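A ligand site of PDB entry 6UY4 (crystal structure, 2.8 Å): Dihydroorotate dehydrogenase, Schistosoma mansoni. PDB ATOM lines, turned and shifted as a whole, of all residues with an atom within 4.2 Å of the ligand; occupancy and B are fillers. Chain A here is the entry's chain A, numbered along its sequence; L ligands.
N of Ala 90 lies close to O3 of the ligand (3.5 Å).
An oxygen (O3) of the ligand sits at hydrogen-bond distance from the backbone carbonyl oxygen of Ala 90 (2.5 Å).
An oxygen (O7) of the ligand is in hydrogen-bond range of the backbone NH (N) of Gly 304 (2.7 Å).
ND2 of Asn 200 sits at hydrogen-bond distance from O1 of the ligand (2.7 Å).
The backbone NH of Thr 114 is in hydrogen-bond range of an oxygen (O2) of the ligand, at 3.2 Å.
OG1 of Thr 114 sits at hydrogen-bond distance from N2 of the ligand, 2.7 Å away.
The backbone NH (N) of Thr 355 lies within hydrogen-bond range of an oxygen (O9) of the ligand.
An oxygen (O9) of the ligand lies within hydrogen-bond range of the side-chain hydroxyl (OG1) of Thr 355.
An oxygen (O7) of the ligand sits at hydrogen-bond distance from the backbone NH of Gly 333 (2.9 Å).
The side-chain amino group (NZ) of Lys 241 lies within hydrogen-bond range of an oxygen (O4) of the ligand, at 3.0 Å.
The backbone NH (N) of Tyr 354 lies close to an oxygen (O9) of the ligand.
The backbone carbonyl oxygen of Ser 271 is in hydrogen-bond range of an oxygen (O4) of the ligand, 3.3 Å away.
The backbone NH of Gly 332 lies close to an oxygen (O8) of the ligand, at 3.4 Å.
An oxygen (O1) of the ligand lies within hydrogen-bond range of the side-chain amide nitrogen (ND2) of Asn 169 (3.4 Å).
The side-chain hydroxyl of Thr 355 lies within hydrogen-bond range of the backbone NH of Gly 304, 3.5 Å away.
The side-chain hydroxyl of Tyr 354 is in hydrogen-bond range of the backbone carbonyl oxygen of Gly 91, 3.1 Å away.
The backbone carbonyl oxygen (O) of Gly 113 sits at hydrogen-bond distance from the backbone NH (N) of Gly 91, 2.9 Å away.
N of Ser 271 sits at hydrogen-bond distance from O of Val 331, 3.0 Å away.
N of Cys 141 lies within hydrogen-bond range of OD1 of Asn 139 (3.4 Å).
The side-chain amide oxygen (OD1) of Asn 272 sits at hydrogen-bond distance from the side-chain hydroxyl (OG1) of Thr 273.
O of Val 137 is in hydrogen-bond range of N of Ser 303 (2.8 Å).
N of Ala 89 lies within hydrogen-bond range of O of Leu 353, at 3.0 Å.
CB of Ala 89 touches O3 of the ligand, at 3.4 Å.
CA of Gly 91 touches N3 of the ligand, 3.2 Å away.
Lys 94 touches the ligand (NZ to N3, 3.5 Å).
ND2 of Asn 139 touches C8 of the ligand, at 3.3 Å.
Asn 272 touches the ligand (OD1 to C13, 3.4 Å).
Ser 303 touches the ligand (OG to C9, 3.4 Å).
Leu 307 touches the ligand.
CG1 of Val 331 touches C17 of the ligand, 3.5 Å away.
Leu 353 touches the ligand (CA to O8, 3.7 Å).
Hydrophobic or aromatic side chains within 4 Å of the ligand: Ala 89, Ala 90, Leu 307, Val 331 and Tyr 354.
Of the 27 residues printed, 20 come within 4 Å of the ligand.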
ATOM      1  N   ALA A  89      22.500 -32.265  27.486  1.00  0.00           N
ATOM      2  CA  ALA A  89      21.193 -31.635  27.509  1.00  0.00           C
ATOM      3  C   ALA A  89      20.352 -32.095  26.315  1.00  0.00           C
ATOM      4  O   ALA A  89      20.836 -32.739  25.384  1.00  0.00           O
ATOM      5  CB  ALA A  89      21.323 -30.117  27.502  1.00  0.00           C
ATOM      6  N   ALA A  90      19.070 -31.755  26.360  1.00  0.00           N
ATOM      7  CA  ALA A  90      18.154 -32.135  25.297  1.00  0.00           C
ATOM      8  C   ALA A  90      18.454 -31.352  24.026  1.00  0.00           C
ATOM      9  O   ALA A  90      19.070 -30.284  24.036  1.00  0.00           O
ATOM     10  CB  ALA A  90      16.703 -31.901  25.735  1.00  0.00           C
ATOM     11  N   GLY A  91      17.999 -31.906  22.902  1.00  0.00           N
ATOM     12  CA  GLY A  91      18.139 -31.275  21.601  1.00  0.00           C
ATOM     13  C   GLY A  91      19.228 -31.839  20.730  1.00  0.00           C
ATOM     14  O   GLY A  91      19.230 -31.586  19.520  1.00  0.00           O
ATOM     15  N   LYS A  94      17.766 -35.845  19.433  1.00  0.00           N
ATOM     16  CA  LYS A  94      16.337 -35.558  19.379  1.00  0.00           C
ATOM     17  C   LYS A  94      15.513 -36.819  19.174  1.00  0.00           C
ATOM     18  O   LYS A  94      14.372 -36.896  19.647  1.00  0.00           O
ATOM     19  CB  LYS A  94      16.048 -34.571  18.245  1.00  0.00           C
ATOM     20  CG  LYS A  94      16.661 -33.197  18.408  1.00  0.00           C
ATOM     21  CD  LYS A  94      16.478 -32.365  17.148  1.00  0.00           C
ATOM     22  CE  LYS A  94      16.963 -30.940  17.343  1.00  0.00           C
ATOM     23  NZ  LYS A  94      16.152 -30.213  18.357  1.00  0.00           N
ATOM     24  N   GLY A 113      15.232 -35.992  23.244  1.00  0.00           N
ATOM     25  CA  GLY A 113      14.172 -35.031  23.016  1.00  0.00           C
ATOM     26  C   GLY A 113      14.674 -33.798  22.304  1.00  0.00           C
ATOM     27  O   GLY A 113      15.869 -33.686  22.024  1.00  0.00           O
ATOM     28  N   THR A 114      13.784 -32.840  22.016  1.00  0.00           N
ATOM     29  CA  THR A 114      12.378 -32.913  22.405  1.00  0.00           C
ATOM     30  C   THR A 114      11.550 -33.742  21.413  1.00  0.00           C
ATOM     31  O   THR A 114      11.686 -33.582  20.198  1.00  0.00           O
ATOM     32  CB  THR A 114      11.773 -31.499  22.506  1.00  0.00           C
ATOM     33  OG1 THR A 114      12.333 -30.818  23.638  1.00  0.00           O
ATOM     34  CG2 THR A 114      10.266 -31.557  22.651  1.00  0.00           C
ATOM     35  N   ILE A 128      20.200 -23.085  12.258  1.00  0.00           N
ATOM     36  CA  ILE A 128      21.284 -23.223  13.216  1.00  0.00           C
ATOM     37  C   ILE A 128      22.466 -22.397  12.725  1.00  0.00           C
ATOM     38  O   ILE A 128      22.856 -22.512  11.558  1.00  0.00           O
ATOM     39  CB  ILE A 128      21.695 -24.693  13.418  1.00  0.00           C
ATOM     40  CG1 ILE A 128      20.591 -25.478  14.121  1.00  0.00           C
ATOM     41  CG2 ILE A 128      22.981 -24.772  14.207  1.00  0.00           C
ATOM     42  CD1 ILE A 128      20.923 -26.937  14.348  1.00  0.00           C
ATOM     43  N   VAL A 137      26.015 -20.545  20.061  1.00  0.00           N
ATOM     44  CA  VAL A 137      25.173 -21.033  18.984  1.00  0.00           C
ATOM     45  C   VAL A 137      23.803 -20.365  19.093  1.00  0.00           C
ATOM     46  O   VAL A 137      23.248 -20.241  20.198  1.00  0.00           O
ATOM     47  CB  VAL A 137      25.025 -22.571  19.022  1.00  0.00           C
ATOM     48  CG1 VAL A 137      24.023 -23.052  17.976  1.00  0.00           C
ATOM     49  CG2 VAL A 137      26.371 -23.250  18.803  1.00  0.00           C
ATOM     50  N   ASN A 139      19.991 -20.862  17.542  1.00  0.00           N
ATOM     51  CA  ASN A 139      19.172 -21.855  16.852  1.00  0.00           C
ATOM     52  C   ASN A 139      17.697 -21.492  16.950  1.00  0.00           C
ATOM     53  O   ASN A 139      17.261 -20.874  17.931  1.00  0.00           O
ATOM     54  CB  ASN A 139      19.398 -23.263  17.423  1.00  0.00           C
ATOM     55  CG  ASN A 139      18.463 -23.578  18.592  1.00  0.00           C
ATOM     56  OD1 ASN A 139      17.385 -24.134  18.399  1.00  0.00           O
ATOM     57  ND2 ASN A 139      18.888 -23.228  19.796  1.00  0.00           N
ATOM     58  N   CYS A 141      15.238 -24.179  15.761  1.00  0.00           N
ATOM     59  CA  CYS A 141      14.842 -25.433  15.130  1.00  0.00           C
ATOM     60  C   CYS A 141      13.321 -25.582  15.114  1.00  0.00           C
ATOM     61  O   CYS A 141      12.730 -25.862  14.063  1.00  0.00           O
ATOM     62  CB  CYS A 141      15.490 -26.611  15.855  1.00  0.00           C
ATOM     63  SG  CYS A 141      17.294 -26.579  15.873  1.00  0.00           S
ATOM     64  N   PHE A 143      11.384 -27.700  17.309  1.00  0.00           N
ATOM     65  CA  PHE A 143      10.946 -29.059  17.660  1.00  0.00           C
ATOM     66  C   PHE A 143      10.762 -29.924  16.403  1.00  0.00           C
ATOM     67  O   PHE A 143       9.650 -30.220  15.978  1.00  0.00           O
ATOM     68  CB  PHE A 143       9.658 -29.027  18.493  1.00  0.00           C
ATOM     69  CG  PHE A 143       9.834 -28.420  19.864  1.00  0.00           C
ATOM     70  CD1 PHE A 143       8.721 -28.081  20.618  1.00  0.00           C
ATOM     71  CD2 PHE A 143      11.087 -28.206  20.395  1.00  0.00           C
ATOM     72  CE1 PHE A 143       8.870 -27.534  21.882  1.00  0.00           C
ATOM     73  CE2 PHE A 143      11.242 -27.656  21.652  1.00  0.00           C
ATOM     74  CZ  PHE A 143      10.128 -27.318  22.392  1.00  0.00           C
ATOM     75  N   ASN A 169      12.532 -35.692  26.967  1.00  0.00           N
ATOM     76  CA  ASN A 169      11.966 -34.353  27.003  1.00  0.00           C
ATOM     77  C   ASN A 169      10.751 -34.308  26.085  1.00  0.00           C
ATOM     78  O   ASN A 169      10.874 -34.488  24.871  1.00  0.00           O
ATOM     79  CB  ASN A 169      13.006 -33.317  26.570  1.00  0.00           C
ATOM     80  CG  ASN A 169      12.522 -31.892  26.747  1.00  0.00           C
ATOM     81  OD1 ASN A 169      11.688 -31.405  25.972  1.00  0.00           O
ATOM     82  ND2 ASN A 169      13.029 -31.217  27.762  1.00  0.00           N
ATOM     83  N   ASN A 200       8.953 -28.747  28.918  1.00  0.00           N
ATOM     84  CA  ASN A 200       9.464 -27.401  28.742  1.00  0.00           C
ATOM     85  C   ASN A 200       8.366 -26.373  29.001  1.00  0.00           C
ATOM     86  O   ASN A 200       7.301 -26.427  28.369  1.00  0.00           O
ATOM     87  CB  ASN A 200      10.036 -27.226  27.340  1.00  0.00           C
ATOM     88  CG  ASN A 200      11.372 -27.896  27.156  1.00  0.00           C
ATOM     89  OD1 ASN A 200      11.785 -28.718  27.980  1.00  0.00           O
ATOM     90  ND2 ASN A 200      12.064 -27.563  26.079  1.00  0.00           N
ATOM     91  N   LYS A 241      11.401 -27.833  32.834  1.00  0.00           N
ATOM     92  CA  LYS A 241      12.502 -27.051  32.281  1.00  0.00           C
ATOM     93  C   LYS A 241      11.996 -25.664  31.916  1.00  0.00           C
ATOM     94  O   LYS A 241      11.049 -25.535  31.129  1.00  0.00           O
ATOM     95  CB  LYS A 241      13.111 -27.753  31.071  1.00  0.00           C
ATOM     96  CG  LYS A 241      14.356 -27.082  30.514  1.00  0.00           C
ATOM     97  CD  LYS A 241      14.993 -27.947  29.440  1.00  0.00           C
ATOM     98  CE  LYS A 241      16.260 -27.308  28.899  1.00  0.00           C
ATOM     99  NZ  LYS A 241      16.912 -28.172  27.874  1.00  0.00           N
ATOM    100  N   SER A 271      18.804 -23.690  32.762  1.00  0.00           N
ATOM    101  CA  SER A 271      17.596 -23.307  32.042  1.00  0.00           C
ATOM    102  C   SER A 271      17.742 -23.634  30.557  1.00  0.00           C
ATOM    103  O   SER A 271      18.627 -24.391  30.162  1.00  0.00           O
ATOM    104  CB  SER A 271      17.312 -21.815  32.207  1.00  0.00           C
ATOM    105  OG  SER A 271      18.387 -21.034  31.714  1.00  0.00           O
ATOM    106  N   ASN A 272      16.876 -23.040  29.737  1.00  0.00           N
ATOM    107  CA  ASN A 272      16.952 -23.207  28.289  1.00  0.00           C
ATOM    108  C   ASN A 272      17.774 -22.071  27.688  1.00  0.00           C
ATOM    109  O   ASN A 272      18.722 -21.593  28.311  1.00  0.00           O
ATOM    110  CB  ASN A 272      15.546 -23.263  27.672  1.00  0.00           C
ATOM    111  CG  ASN A 272      15.509 -24.037  26.374  1.00  0.00           C
ATOM    112  OD1 ASN A 272      16.344 -23.838  25.488  1.00  0.00           O
ATOM    113  ND2 ASN A 272      14.536 -24.937  26.240  1.00  0.00           N
ATOM    114  N   THR A 273      17.411 -21.622  26.487  1.00  0.00           N
ATOM    115  CA  THR A 273      18.140 -20.588  25.782  1.00  0.00           C
ATOM    116  C   THR A 273      17.505 -19.210  25.989  1.00  0.00           C
ATOM    117  O   THR A 273      16.340 -19.094  26.378  1.00  0.00           O
ATOM    118  CB  THR A 273      18.228 -20.905  24.285  1.00  0.00           C
ATOM    119  OG1 THR A 273      16.909 -21.043  23.750  1.00  0.00           O
ATOM    120  CG2 THR A 273      19.006 -22.182  24.052  1.00  0.00           C
ATOM    121  N   SER A 303      22.669 -19.962  22.962  1.00  0.00           N
ATOM    122  CA  SER A 303      23.290 -20.895  23.877  1.00  0.00           C
ATOM    123  C   SER A 303      24.805 -20.746  23.787  1.00  0.00           C
ATOM    124  O   SER A 303      25.342 -20.195  22.824  1.00  0.00           O
ATOM    125  CB  SER A 303      22.885 -22.348  23.574  1.00  0.00           C
ATOM    126  OG  SER A 303      23.235 -22.700  22.249  1.00  0.00           O
ATOM    127  N   GLY A 304      25.495 -21.248  24.801  1.00  0.00           N
ATOM    128  CA  GLY A 304      26.940 -21.168  24.865  1.00  0.00           C
ATOM    129  C   GLY A 304      27.403 -20.310  26.033  1.00  0.00           C
ATOM    130  O   GLY A 304      26.651 -19.990  26.959  1.00  0.00           O
ATOM    131  N   LEU A 307      25.657 -17.408  27.822  1.00  0.00           N
ATOM    132  CA  LEU A 307      24.484 -17.758  28.604  1.00  0.00           C
ATOM    133  C   LEU A 307      24.810 -18.083  30.057  1.00  0.00           C
ATOM    134  O   LEU A 307      23.914 -17.990  30.909  1.00  0.00           O
ATOM    135  CB  LEU A 307      23.766 -18.957  27.958  1.00  0.00           C
ATOM    136  CG  LEU A 307      22.509 -19.534  28.620  1.00  0.00           C
ATOM    137  CD1 LEU A 307      21.424 -18.487  28.677  1.00  0.00           C
ATOM    138  CD2 LEU A 307      22.038 -20.772  27.877  1.00  0.00           C
ATOM    139  N   VAL A 331      21.856 -25.975  33.660  1.00  0.00           N
ATOM    140  CA  VAL A 331      22.215 -26.090  32.253  1.00  0.00           C
ATOM    141  C   VAL A 331      22.434 -24.694  31.698  1.00  0.00           C
ATOM    142  O   VAL A 331      21.726 -23.743  32.062  1.00  0.00           O
ATOM    143  CB  VAL A 331      21.130 -26.834  31.432  1.00  0.00           C
ATOM    144  CG1 VAL A 331      21.700 -27.307  30.114  1.00  0.00           C
ATOM    145  CG2 VAL A 331      20.572 -28.003  32.220  1.00  0.00           C
ATOM    146  N   GLY A 332      23.422 -24.552  30.808  1.00  0.00           N
ATOM    147  CA  GLY A 332      23.633 -23.288  30.132  1.00  0.00           C
ATOM    148  C   GLY A 332      25.024 -22.702  30.288  1.00  0.00           C
ATOM    149  O   GLY A 332      25.375 -22.172  31.342  1.00  0.00           O
ATOM    150  N   GLY A 333      25.821 -22.788  29.227  1.00  0.00           N
ATOM    151  CA  GLY A 333      27.107 -22.127  29.196  1.00  0.00           C
ATOM    152  C   GLY A 333      28.225 -22.803  29.945  1.00  0.00           C
ATOM    153  O   GLY A 333      29.233 -22.166  30.248  1.00  0.00           O
ATOM    154  N   ILE A 334      28.090 -24.091  30.255  1.00  0.00           N
ATOM    155  CA  ILE A 334      29.148 -24.833  30.937  1.00  0.00           C
ATOM    156  C   ILE A 334      30.216 -25.171  29.908  1.00  0.00           C
ATOM    157  O   ILE A 334      29.975 -25.967  28.996  1.00  0.00           O
ATOM    158  CB  ILE A 334      28.608 -26.091  31.626  1.00  0.00           C
ATOM    159  CG1 ILE A 334      27.725 -25.707  32.817  1.00  0.00           C
ATOM    160  CG2 ILE A 334      29.760 -26.979  32.075  1.00  0.00           C
ATOM    161  CD1 ILE A 334      27.204 -26.901  33.583  1.00  0.00           C
ATOM    162  N   LEU A 353      25.100 -29.859  29.373  1.00  0.00           N
ATOM    163  CA  LEU A 353      25.755 -28.972  28.417  1.00  0.00           C
ATOM    164  C   LEU A 353      25.333 -29.370  27.004  1.00  0.00           C
ATOM    165  O   LEU A 353      24.712 -30.408  26.784  1.00  0.00           O
ATOM    166  CB  LEU A 353      27.285 -29.010  28.573  1.00  0.00           C
ATOM    167  CG  LEU A 353      27.997 -30.368  28.466  1.00  0.00           C
ATOM    168  CD1 LEU A 353      28.407 -30.678  27.034  1.00  0.00           C
ATOM    169  CD2 LEU A 353      29.200 -30.408  29.392  1.00  0.00           C
ATOM    170  N   TYR A 354      25.707 -28.531  26.050  1.00  0.00           N
ATOM    171  CA  TYR A 354      25.376 -28.763  24.649  1.00  0.00           C
ATOM    172  C   TYR A 354      26.361 -28.030  23.753  1.00  0.00           C
ATOM    173  O   TYR A 354      27.068 -28.655  22.948  1.00  0.00           O
ATOM    174  CB  TYR A 354      23.943 -28.293  24.355  1.00  0.00           C
ATOM    175  CG  TYR A 354      23.373 -28.720  23.019  1.00  0.00           C
ATOM    176  CD1 TYR A 354      22.242 -29.515  22.955  1.00  0.00           C
ATOM    177  CD2 TYR A 354      23.957 -28.322  21.814  1.00  0.00           C
ATOM    178  CE1 TYR A 354      21.710 -29.909  21.748  1.00  0.00           C
ATOM    179  CE2 TYR A 354      23.431 -28.714  20.599  1.00  0.00           C
ATOM    180  CZ  TYR A 354      22.308 -29.512  20.578  1.00  0.00           C
ATOM    181  OH  TYR A 354      21.777 -29.895  19.362  1.00  0.00           O
ATOM    182  N   THR A 355      26.424 -26.700  23.871  1.00  0.00           N
ATOM    183  CA  THR A 355      27.239 -25.911  22.965  1.00  0.00           C
ATOM    184  C   THR A 355      28.721 -26.203  23.144  1.00  0.00           C
ATOM    185  O   THR A 355      29.465 -26.294  22.159  1.00  0.00           O
ATOM    186  CB  THR A 355      26.952 -24.417  23.180  1.00  0.00           C
ATOM    187  OG1 THR A 355      25.563 -24.165  22.949  1.00  0.00           O
ATOM    188  CG2 THR A 355      27.777 -23.578  22.212  1.00  0.00           C
HETATM  189  N1  LIG L   1      16.238 -27.822  24.773  1.00  0.00           N
HETATM  190  C1  LIG L   1      15.097 -28.585  24.920  1.00  0.00           C
HETATM  191  O1  LIG L   1      14.542 -28.663  26.011  1.00  0.00           O
HETATM  192  N2  LIG L   1      14.568 -29.266  23.836  1.00  0.00           N
HETATM  193  C2  LIG L   1      15.197 -29.185  22.605  1.00  0.00           C
HETATM  194  O2  LIG L   1      14.720 -29.790  21.638  1.00  0.00           O
HETATM  195  C3  LIG L   1      16.343 -28.420  22.450  1.00  0.00           C
HETATM  196  N3  LIG L   1      16.961 -28.334  21.226  1.00  0.00           N
HETATM  197  C4  LIG L   1      18.101 -27.572  21.079  1.00  0.00           C
HETATM  198  C5  LIG L   1      18.723 -27.496  19.842  1.00  0.00           C
HETATM  199  C6  LIG L   1      19.874 -26.727  19.679  1.00  0.00           C
HETATM  200  C7  LIG L   1      20.538 -26.643  18.346  1.00  0.00           C
HETATM  201  C8  LIG L   1      20.410 -26.042  20.769  1.00  0.00           C
HETATM  202  C9  LIG L   1      21.645 -25.220  20.610  1.00  0.00           C
HETATM  203  C10 LIG L   1      19.782 -26.121  22.015  1.00  0.00           C
HETATM  204  C11 LIG L   1      18.631 -26.889  22.177  1.00  0.00           C
HETATM  205  N4  LIG L   1      18.007 -26.978  23.409  1.00  0.00           N
HETATM  206  C12 LIG L   1      16.861 -27.733  23.541  1.00  0.00           C
HETATM  207  C13 LIG L   1      18.551 -26.245  24.600  1.00  0.00           C
HETATM  208  C14 LIG L   1      19.588 -27.093  25.316  1.00  0.00           C
HETATM  209  O3  LIG L   1      19.033 -28.349  25.649  1.00  0.00           O
HETATM  210  C15 LIG L   1      20.052 -26.416  26.596  1.00  0.00           C
HETATM  211  O4  LIG L   1      18.930 -26.057  27.378  1.00  0.00           O
HETATM  212  C16 LIG L   1      20.888 -25.168  26.317  1.00  0.00           C
HETATM  213  O5  LIG L   1      21.476 -25.234  25.040  1.00  0.00           O
HETATM  214  C17 LIG L   1      21.979 -25.080  27.379  1.00  0.00           C
HETATM  215  O6  LIG L   1      22.934 -24.105  27.029  1.00  0.00           O
HETATM  216  P1  LIG L   1      24.435 -24.583  26.714  1.00  0.00           P
HETATM  217  O7  LIG L   1      25.264 -23.351  26.437  1.00  0.00           O
HETATM  218  O8  LIG L   1      24.998 -25.359  27.880  1.00  0.00           O
HETATM  219  O9  LIG L   1      24.415 -25.450  25.482  1.00  0.00           O
